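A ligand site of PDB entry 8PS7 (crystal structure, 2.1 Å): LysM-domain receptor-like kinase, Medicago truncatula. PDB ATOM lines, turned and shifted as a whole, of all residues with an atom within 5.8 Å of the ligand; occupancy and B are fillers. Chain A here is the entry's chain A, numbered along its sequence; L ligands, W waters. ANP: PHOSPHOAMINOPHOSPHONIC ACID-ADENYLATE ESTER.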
ATOM      1  N   LYS A  22      31.228   6.382 -18.282  1.00  0.00           N
ATOM      2  CA  LYS A  22      31.131   5.952 -19.666  1.00  0.00           C
ATOM      3  C   LYS A  22      32.537   5.910 -20.268  1.00  0.00           C
ATOM      4  O   LYS A  22      33.540   6.212 -19.604  1.00  0.00           O
ATOM      5  CB  LYS A  22      30.198   6.875 -20.443  1.00  0.00           C
ATOM      6  CG  LYS A  22      28.730   6.433 -20.432  1.00  0.00           C
ATOM      7  CD  LYS A  22      28.507   5.307 -21.428  1.00  0.00           C
ATOM      8  CE  LYS A  22      27.160   5.448 -22.129  1.00  0.00           C
ATOM      9  NZ  LYS A  22      25.995   5.099 -21.260  1.00  0.00           N
ATOM     10  N   ILE A  23      32.617   5.542 -21.549  1.00  0.00           N
ATOM     11  CA  ILE A  23      33.910   5.282 -22.174  1.00  0.00           C
ATOM     12  C   ILE A  23      34.858   6.453 -21.968  1.00  0.00           C
ATOM     13  O   ILE A  23      35.962   6.304 -21.436  1.00  0.00           O
ATOM     14  CB  ILE A  23      33.729   4.948 -23.664  1.00  0.00           C
ATOM     15  CG1 ILE A  23      32.798   3.744 -23.827  1.00  0.00           C
ATOM     16  CG2 ILE A  23      35.089   4.674 -24.306  1.00  0.00           C
ATOM     17  CD1 ILE A  23      33.144   2.862 -25.001  1.00  0.00           C
ATOM     18  N   LYS A  24      34.438   7.650 -22.391  1.00  0.00           N
ATOM     19  CA  LYS A  24      35.290   8.823 -22.274  1.00  0.00           C
ATOM     20  C   LYS A  24      35.755   9.014 -20.837  1.00  0.00           C
ATOM     21  O   LYS A  24      34.968   8.905 -19.897  1.00  0.00           O
ATOM     22  CB  LYS A  24      34.559  10.069 -22.758  1.00  0.00           C
ATOM     23  CG  LYS A  24      35.372  11.347 -22.716  1.00  0.00           C
ATOM     24  CD  LYS A  24      36.070  11.626 -24.038  1.00  0.00           C
ATOM     25  CE  LYS A  24      36.616  13.057 -24.086  1.00  0.00           C
ATOM     26  NZ  LYS A  24      37.750  13.279 -23.151  1.00  0.00           N
ATOM     27  N   SER A  26      36.444  11.687 -19.340  1.00  0.00           N
ATOM     28  CA  SER A  26      35.740  12.836 -18.756  1.00  0.00           C
ATOM     29  C   SER A  26      34.239  12.621 -18.610  1.00  0.00           C
ATOM     30  O   SER A  26      33.568  13.455 -18.000  1.00  0.00           O
ATOM     31  CB  SER A  26      36.000  14.090 -19.594  1.00  0.00           C
ATOM     32  OG  SER A  26      35.820  13.838 -20.978  1.00  0.00           O
ATOM     33  N   VAL A  27      33.704  11.534 -19.143  1.00  0.00           N
ATOM     34  CA  VAL A  27      32.264  11.301 -19.190  1.00  0.00           C
ATOM     35  C   VAL A  27      31.892  10.272 -18.133  1.00  0.00           C
ATOM     36  O   VAL A  27      32.339   9.117 -18.187  1.00  0.00           O
ATOM     37  CB  VAL A  27      31.815  10.831 -20.589  1.00  0.00           C
ATOM     38  CG1 VAL A  27      30.334  10.493 -20.573  1.00  0.00           C
ATOM     39  CG2 VAL A  27      32.113  11.911 -21.616  1.00  0.00           C
ATOM     40  N   ALA A  38      24.602  12.891 -17.302  1.00  0.00           N
ATOM     41  CA  ALA A  38      25.987  12.607 -17.652  1.00  0.00           C
ATOM     42  C   ALA A  38      26.852  13.788 -17.239  1.00  0.00           C
ATOM     43  O   ALA A  38      26.518  14.939 -17.548  1.00  0.00           O
ATOM     44  CB  ALA A  38      26.140  12.327 -19.148  1.00  0.00           C
ATOM     45  N   LYS A  40      30.548  15.610 -17.420  1.00  0.00           N
ATOM     46  CA  LYS A  40      31.781  15.743 -18.187  1.00  0.00           C
ATOM     47  C   LYS A  40      32.743  16.647 -17.421  1.00  0.00           C
ATOM     48  O   LYS A  40      32.415  17.798 -17.135  1.00  0.00           O
ATOM     49  CB  LYS A  40      31.503  16.314 -19.579  1.00  0.00           C
ATOM     50  CG  LYS A  40      32.744  16.851 -20.268  1.00  0.00           C
ATOM     51  CD  LYS A  40      32.394  17.552 -21.579  1.00  0.00           C
ATOM     52  CE  LYS A  40      32.027  16.544 -22.650  1.00  0.00           C
ATOM     53  NZ  LYS A  40      33.173  15.647 -22.975  1.00  0.00           N
ATOM     54  N   ILE A  62      21.819  17.532 -27.340  1.00  0.00           N
ATOM     55  CA  ILE A  62      22.042  17.108 -25.966  1.00  0.00           C
ATOM     56  C   ILE A  62      21.951  18.317 -25.040  1.00  0.00           C
ATOM     57  O   ILE A  62      22.712  19.279 -25.167  1.00  0.00           O
ATOM     58  CB  ILE A  62      23.387  16.382 -25.841  1.00  0.00           C
ATOM     59  CG1 ILE A  62      23.421  15.534 -24.558  1.00  0.00           C
ATOM     60  CG2 ILE A  62      24.547  17.363 -25.869  1.00  0.00           C
ATOM     61  CD1 ILE A  62      22.364  14.451 -24.520  1.00  0.00           C
ATOM     62  N   TYR A  78      24.891  17.065 -18.451  1.00  0.00           N
ATOM     63  CA  TYR A  78      23.970  16.990 -19.568  1.00  0.00           C
ATOM     64  C   TYR A  78      22.873  15.982 -19.272  1.00  0.00           C
ATOM     65  O   TYR A  78      22.963  15.171 -18.344  1.00  0.00           O
ATOM     66  CB  TYR A  78      24.701  16.597 -20.857  1.00  0.00           C
ATOM     67  CG  TYR A  78      25.792  17.546 -21.296  1.00  0.00           C
ATOM     68  CD1 TYR A  78      27.044  17.509 -20.699  1.00  0.00           C
ATOM     69  CD2 TYR A  78      25.573  18.469 -22.309  1.00  0.00           C
ATOM     70  CE1 TYR A  78      28.045  18.373 -21.097  1.00  0.00           C
ATOM     71  CE2 TYR A  78      26.573  19.333 -22.707  1.00  0.00           C
ATOM     72  CZ  TYR A  78      27.803  19.288 -22.096  1.00  0.00           C
ATOM     73  OH  TYR A  78      28.805  20.142 -22.497  1.00  0.00           O
ATOM     74  N   GLU A  79      21.814  16.028 -20.072  1.00  0.00           N
ATOM     75  CA  GLU A  79      20.781  15.008 -19.986  1.00  0.00           C
ATOM     76  C   GLU A  79      21.364  13.665 -20.414  1.00  0.00           C
ATOM     77  O   GLU A  79      22.066  13.580 -21.429  1.00  0.00           O
ATOM     78  CB  GLU A  79      19.586  15.368 -20.863  1.00  0.00           C
ATOM     79  CG  GLU A  79      19.890  15.521 -22.346  1.00  0.00           C
ATOM     80  CD  GLU A  79      18.640  15.529 -23.200  1.00  0.00           C
ATOM     81  OE1 GLU A  79      17.708  14.751 -22.889  1.00  0.00           O
ATOM     82  OE2 GLU A  79      18.574  16.305 -24.170  1.00  0.00           O
ATOM     83  N   PHE A  80      21.089  12.633 -19.635  1.00  0.00           N
ATOM     84  CA  PHE A  80      21.608  11.302 -19.949  1.00  0.00           C
ATOM     85  C   PHE A  80      20.853  10.722 -21.133  1.00  0.00           C
ATOM     86  O   PHE A  80      19.616  10.765 -21.185  1.00  0.00           O
ATOM     87  CB  PHE A  80      21.480  10.384 -18.738  1.00  0.00           C
ATOM     88  CG  PHE A  80      21.965   8.984 -18.996  1.00  0.00           C
ATOM     89  CD1 PHE A  80      23.322   8.719 -19.107  1.00  0.00           C
ATOM     90  CD2 PHE A  80      21.078   7.934 -19.115  1.00  0.00           C
ATOM     91  CE1 PHE A  80      23.779   7.437 -19.347  1.00  0.00           C
ATOM     92  CE2 PHE A  80      21.526   6.651 -19.357  1.00  0.00           C
ATOM     93  CZ  PHE A  80      22.879   6.404 -19.461  1.00  0.00           C
ATOM     94  N   ALA A  81      21.599  10.186 -22.096  1.00  0.00           N
ATOM     95  CA  ALA A  81      21.036   9.572 -23.296  1.00  0.00           C
ATOM     96  C   ALA A  81      21.277   8.078 -23.196  1.00  0.00           C
ATOM     97  O   ALA A  81      22.364   7.587 -23.518  1.00  0.00           O
ATOM     98  CB  ALA A  81      21.652  10.168 -24.554  1.00  0.00           C
ATOM     99  N   GLU A  82      20.260   7.341 -22.742  1.00  0.00           N
ATOM    100  CA  GLU A  82      20.321   5.900 -22.799  1.00  0.00           C
ATOM    101  C   GLU A  82      20.199   5.433 -24.245  1.00  0.00           C
ATOM    102  O   GLU A  82      19.545   6.081 -25.071  1.00  0.00           O
ATOM    103  CB  GLU A  82      19.213   5.278 -21.949  1.00  0.00           C
ATOM    104  CG  GLU A  82      17.818   5.484 -22.493  1.00  0.00           C
ATOM    105  CD  GLU A  82      16.771   4.651 -21.777  1.00  0.00           C
ATOM    106  OE1 GLU A  82      16.748   4.686 -20.527  1.00  0.00           O
ATOM    107  OE2 GLU A  82      15.982   3.965 -22.457  1.00  0.00           O
ATOM    108  N   ASN A  84      22.932   5.103 -25.995  1.00  0.00           N
ATOM    109  CA  ASN A  84      24.307   5.414 -26.393  1.00  0.00           C
ATOM    110  C   ASN A  84      24.295   6.167 -27.730  1.00  0.00           C
ATOM    111  O   ASN A  84      23.487   7.093 -27.893  1.00  0.00           O
ATOM    112  CB  ASN A  84      25.131   4.120 -26.399  1.00  0.00           C
ATOM    113  CG  ASN A  84      24.754   3.201 -25.226  1.00  0.00           C
ATOM    114  OD1 ASN A  84      25.101   3.466 -24.070  1.00  0.00           O
ATOM    115  ND2 ASN A  84      24.017   2.120 -25.517  1.00  0.00           N
ATOM    116  N   SER A  85      25.159   5.808 -28.673  1.00  0.00           N
ATOM    117  CA  SER A  85      25.407   6.530 -29.907  1.00  0.00           C
ATOM    118  C   SER A  85      24.930   5.704 -31.099  1.00  0.00           C
ATOM    119  O   SER A  85      24.870   4.466 -31.034  1.00  0.00           O
ATOM    120  CB  SER A  85      26.903   6.840 -30.082  1.00  0.00           C
ATOM    121  OG  SER A  85      27.589   5.740 -30.661  1.00  0.00           O
ATOM    122  N   ASP A  88      27.201   2.859 -32.202  1.00  0.00           N
ATOM    123  CA  ASP A  88      27.062   1.608 -31.463  1.00  0.00           C
ATOM    124  C   ASP A  88      25.985   0.713 -32.070  1.00  0.00           C
ATOM    125  O   ASP A  88      26.149  -0.505 -32.158  1.00  0.00           O
ATOM    126  CB  ASP A  88      26.750   1.901 -29.998  1.00  0.00           C
ATOM    127  CG  ASP A  88      27.800   2.763 -29.342  1.00  0.00           C
ATOM    128  OD1 ASP A  88      29.003   2.480 -29.547  1.00  0.00           O
ATOM    129  OD2 ASP A  88      27.443   3.716 -28.628  1.00  0.00           O
ATOM    130  N   LYS A 139      29.131  13.235 -36.297  1.00  0.00           N
ATOM    131  CA  LYS A 139      29.483  11.857 -36.567  1.00  0.00           C
ATOM    132  C   LYS A 139      28.453  10.939 -35.935  1.00  0.00           C
ATOM    133  O   LYS A 139      27.724  11.321 -35.017  1.00  0.00           O
ATOM    134  CB  LYS A 139      30.887  11.519 -36.040  1.00  0.00           C
ATOM    135  CG  LYS A 139      31.997  12.402 -36.587  1.00  0.00           C
ATOM    136  CD  LYS A 139      33.269  12.247 -35.762  1.00  0.00           C
ATOM    137  CE  LYS A 139      34.487  12.751 -36.521  1.00  0.00           C
ATOM    138  NZ  LYS A 139      34.329  14.152 -36.989  1.00  0.00           N
ATOM    139  N   GLY A 141      29.077   8.542 -33.990  1.00  0.00           N
ATOM    140  CA  GLY A 141      29.448   8.387 -32.601  1.00  0.00           C
ATOM    141  C   GLY A 141      29.064   9.545 -31.716  1.00  0.00           C
ATOM    142  O   GLY A 141      28.967   9.383 -30.497  1.00  0.00           O
ATOM    143  N   ASN A 142      28.825  10.719 -32.315  1.00  0.00           N
ATOM    144  CA  ASN A 142      28.393  11.892 -31.562  1.00  0.00           C
ATOM    145  C   ASN A 142      26.884  12.034 -31.488  1.00  0.00           C
ATOM    146  O   ASN A 142      26.381  12.758 -30.624  1.00  0.00           O
ATOM    147  CB  ASN A 142      28.976  13.173 -32.179  1.00  0.00           C
ATOM    148  CG  ASN A 142      30.497  13.209 -32.108  1.00  0.00           C
ATOM    149  OD1 ASN A 142      31.086  12.866 -31.080  1.00  0.00           O
ATOM    150  ND2 ASN A 142      31.122  13.628 -33.194  1.00  0.00           N
ATOM    151  N   LEU A 144      23.692  10.935 -30.237  1.00  0.00           N
ATOM    152  CA  LEU A 144      23.168  10.085 -29.190  1.00  0.00           C
ATOM    153  C   LEU A 144      21.694   9.778 -29.442  1.00  0.00           C
ATOM    154  O   LEU A 144      21.032  10.402 -30.268  1.00  0.00           O
ATOM    155  CB  LEU A 144      23.343  10.738 -27.818  1.00  0.00           C
ATOM    156  CG  LEU A 144      24.787  11.095 -27.444  1.00  0.00           C
ATOM    157  CD1 LEU A 144      24.864  11.640 -26.029  1.00  0.00           C
ATOM    158  CD2 LEU A 144      25.704   9.900 -27.624  1.00  0.00           C
ATOM    159  N   SER A 154      25.716  16.033 -29.860  1.00  0.00           N
ATOM    160  CA  SER A 154      26.492  16.208 -28.641  1.00  0.00           C
ATOM    161  C   SER A 154      27.761  17.035 -28.818  1.00  0.00           C
ATOM    162  O   SER A 154      27.848  18.173 -28.334  1.00  0.00           O
ATOM    163  CB  SER A 154      26.857  14.846 -28.051  1.00  0.00           C
ATOM    164  OG  SER A 154      27.806  14.167 -28.864  1.00  0.00           O
ATOM    165  N   ASN A 155      28.772  16.483 -29.499  1.00  0.00           N
ATOM    166  CA  ASN A 155      30.118  17.072 -29.505  1.00  0.00           C
ATOM    167  C   ASN A 155      30.198  18.220 -30.507  1.00  0.00           C
ATOM    168  O   ASN A 155      30.922  18.175 -31.504  1.00  0.00           O
ATOM    169  CB  ASN A 155      31.158  16.008 -29.812  1.00  0.00           C
ATOM    170  CG  ASN A 155      31.410  15.068 -28.639  1.00  0.00           C
ATOM    171  OD1 ASN A 155      30.566  14.923 -27.752  1.00  0.00           O
ATOM    172  ND2 ASN A 155      32.573  14.423 -28.630  1.00  0.00           N
ATOM    173  N   ARG A 175      42.813   7.992 -34.472  1.00  0.00           N
ATOM    174  CA  ARG A 175      41.357   7.978 -34.416  1.00  0.00           C
ATOM    175  C   ARG A 175      40.764   9.283 -34.965  1.00  0.00           C
ATOM    176  O   ARG A 175      39.830   9.250 -35.777  1.00  0.00           O
ATOM    177  CB  ARG A 175      40.908   7.738 -32.978  1.00  0.00           C
ATOM    178  CG  ARG A 175      39.414   7.562 -32.784  1.00  0.00           C
ATOM    179  CD  ARG A 175      39.137   7.054 -31.377  1.00  0.00           C
ATOM    180  NE  ARG A 175      37.797   7.387 -30.926  1.00  0.00           N
ATOM    181  CZ  ARG A 175      37.471   8.524 -30.322  1.00  0.00           C
ATOM    182  NH1 ARG A 175      38.371   9.466 -30.101  1.00  0.00           N
ATOM    183  NH2 ARG A 175      36.220   8.722 -29.929  1.00  0.00           N
HETATM  184  PG  ANP L   1      32.353   8.881 -29.354  1.00  0.00           P
HETATM  185  O1G ANP L   1      33.491   7.937 -29.084  1.00  0.00           O
HETATM  186  O2G ANP L   1      30.990   8.097 -29.197  1.00  0.00           O
HETATM  187  O3G ANP L   1      32.448   9.416 -30.843  1.00  0.00           O
HETATM  188  PB  ANP L   1      33.894  10.616 -27.757  1.00  0.00           P
HETATM  189  O1B ANP L   1      34.745   9.386 -27.626  1.00  0.00           O
HETATM  190  O2B ANP L   1      34.540  11.563 -28.803  1.00  0.00           O
HETATM  191  N3B ANP L   1      32.364  10.261 -28.369  1.00  0.00           N
HETATM  192  PA  ANP L   1      32.572  11.756 -25.532  1.00  0.00           P
HETATM  193  O1A ANP L   1      32.896  12.801 -24.529  1.00  0.00           O
HETATM  194  O2A ANP L   1      31.521  12.182 -26.556  1.00  0.00           O
HETATM  195  O3A ANP L   1      33.883  11.331 -26.357  1.00  0.00           O
HETATM  196  O5' ANP L   1      32.120  10.460 -24.739  1.00  0.00           O
HETATM  197  C5' ANP L   1      31.693   9.360 -25.551  1.00  0.00           C
HETATM  198  C4' ANP L   1      31.058   8.268 -24.731  1.00  0.00           C
HETATM  199  O4' ANP L   1      30.278   8.853 -23.679  1.00  0.00           O
HETATM  200  C3' ANP L   1      30.110   7.391 -25.538  1.00  0.00           C
HETATM  201  O3' ANP L   1      30.111   6.041 -25.085  1.00  0.00           O
HETATM  202  C2' ANP L   1      28.765   8.087 -25.329  1.00  0.00           C
HETATM  203  O2' ANP L   1      27.659   7.192 -25.423  1.00  0.00           O
HETATM  204  C1' ANP L   1      28.903   8.604 -23.894  1.00  0.00           C
HETATM  205  N9  ANP L   1      28.160   9.835 -23.631  1.00  0.00           N
HETATM  206  C8  ANP L   1      28.592  11.123 -23.793  1.00  0.00           C
HETATM  207  N7  ANP L   1      27.713  12.031 -23.477  1.00  0.00           N
HETATM  208  C5  ANP L   1      26.613  11.282 -23.062  1.00  0.00           C
HETATM  209  C6  ANP L   1      25.337  11.651 -22.587  1.00  0.00           C
HETATM  210  N6  ANP L   1      24.932  12.912 -22.444  1.00  0.00           N
HETATM  211  N1  ANP L   1      24.479  10.656 -22.261  1.00  0.00           N
HETATM  212  C2  ANP L   1      24.884   9.395 -22.404  1.00  0.00           C
HETATM  213  N3  ANP L   1      26.051   8.925 -22.835  1.00  0.00           N
HETATM  214  C4  ANP L   1      26.884   9.933 -23.150  1.00  0.00           C
HETATM  215  O   HOH W   1      33.810  13.491 -31.436  1.00  0.00           O
HETATM  216  O   HOH W   2      36.353  13.540 -27.537  1.00  0.00           O
HETATM  217  O   HOH W   3      29.414  10.184 -27.981  1.00  0.00           O
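CE of Lys 22 touches N3 of the ligand, 3.7 Å away.
Ile 23 touches the ligand.
CB of Lys 24 touches O5' of the ligand (3.2 Å).
CG2 of Val 27 touches O1A of the ligand, at 3.1 Å.
Ala 38 touches the ligand (CB to N6, 3.6 Å).
Ile 62 touches the ligand (CD1 to N6, 3.6 Å).
CD1 of Phe 80 touches C2 of the ligand (3.7 Å).
CA of Asn 84 touches O2' of the ligand, at 3.9 Å.
Asn 142 touches the ligand (OD1 to O3G, 3.7 Å).
Leu 144 touches the ligand (CD1 to C5, 3.5 Å).
16 residues have an atom within 4 Å of the ligand: Lys 22, Ile 23, Lys 24, Val 27, Ala 38, Lys 40, Ile 62, Glu 79, Phe 80, Ala 81, Asn 84, Gly 141, Asn 142, Leu 144, Asn 155 and Arg 175.
The nearest printed residue that does not touch the ligand is Tyr 78 (4.02 Å).
Water W3 bridges O of Gly 141 (2.7 Å) and O2G of the ligand (2.9 Å).
Water W1 lies within hydrogen-bond range of the side-chain amide oxygen of Asn 142 (2.8 Å), the side-chain amide nitrogen of Asn 155 (3.2 Å) and an oxygen (O2B) of the ligand (3.3 Å).
OD1 of Asn 142 sits at hydrogen-bond distance from ND2 of Asn 155 (3.3 Å).
OD1 of Asn 155 sits at hydrogen-bond distance from OG of Ser 154 (3.1 Å).
The backbone NH (N) of Lys 22 lies within hydrogen-bond range of the backbone carbonyl oxygen (O) of Val 27 (3.0 Å).
The side-chain amino group (NZ) of Lys 24 lies within hydrogen-bond range of the side-chain hydroxyl (OG) of Ser 26, 3.0 Å away.
The backbone carbonyl oxygen (O) of Ala 38 lies within hydrogen-bond range of the backbone NH (N) of Tyr 78 (2.8 Å).
The backbone carbonyl oxygen (O) of Asn 142 lies within hydrogen-bond range of the side-chain hydroxyl (OG) of Ser 154 (2.7 Å).
NZ of Lys 22 lies within hydrogen-bond range of OD1 of Asn 84, 3.4 Å away.
An oxygen (O2G) of the ligand sits close to the backbone carbonyl oxygen (O) of Gly 141.
The guanidinium group (NH2) of Arg 175 lies within salt-bridge range of an oxygen (O1B) of the ligand.
The backbone NH (N) of Ala 81 sits at hydrogen-bond distance from a nitrogen (N1) of the ligand, at 2.9 Å.
The backbone carbonyl oxygen (O) of Glu 79 is in hydrogen-bond range of a nitrogen (N6) of the ligand, at 3.1 Å.
O2A of the ligand sits close to OD1 of Asn 155 (3.1 Å).
The side-chain amino group (NZ) of Lys 40 lies within salt-bridge range of an oxygen (O1A) of the ligand, 3.3 Å away.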
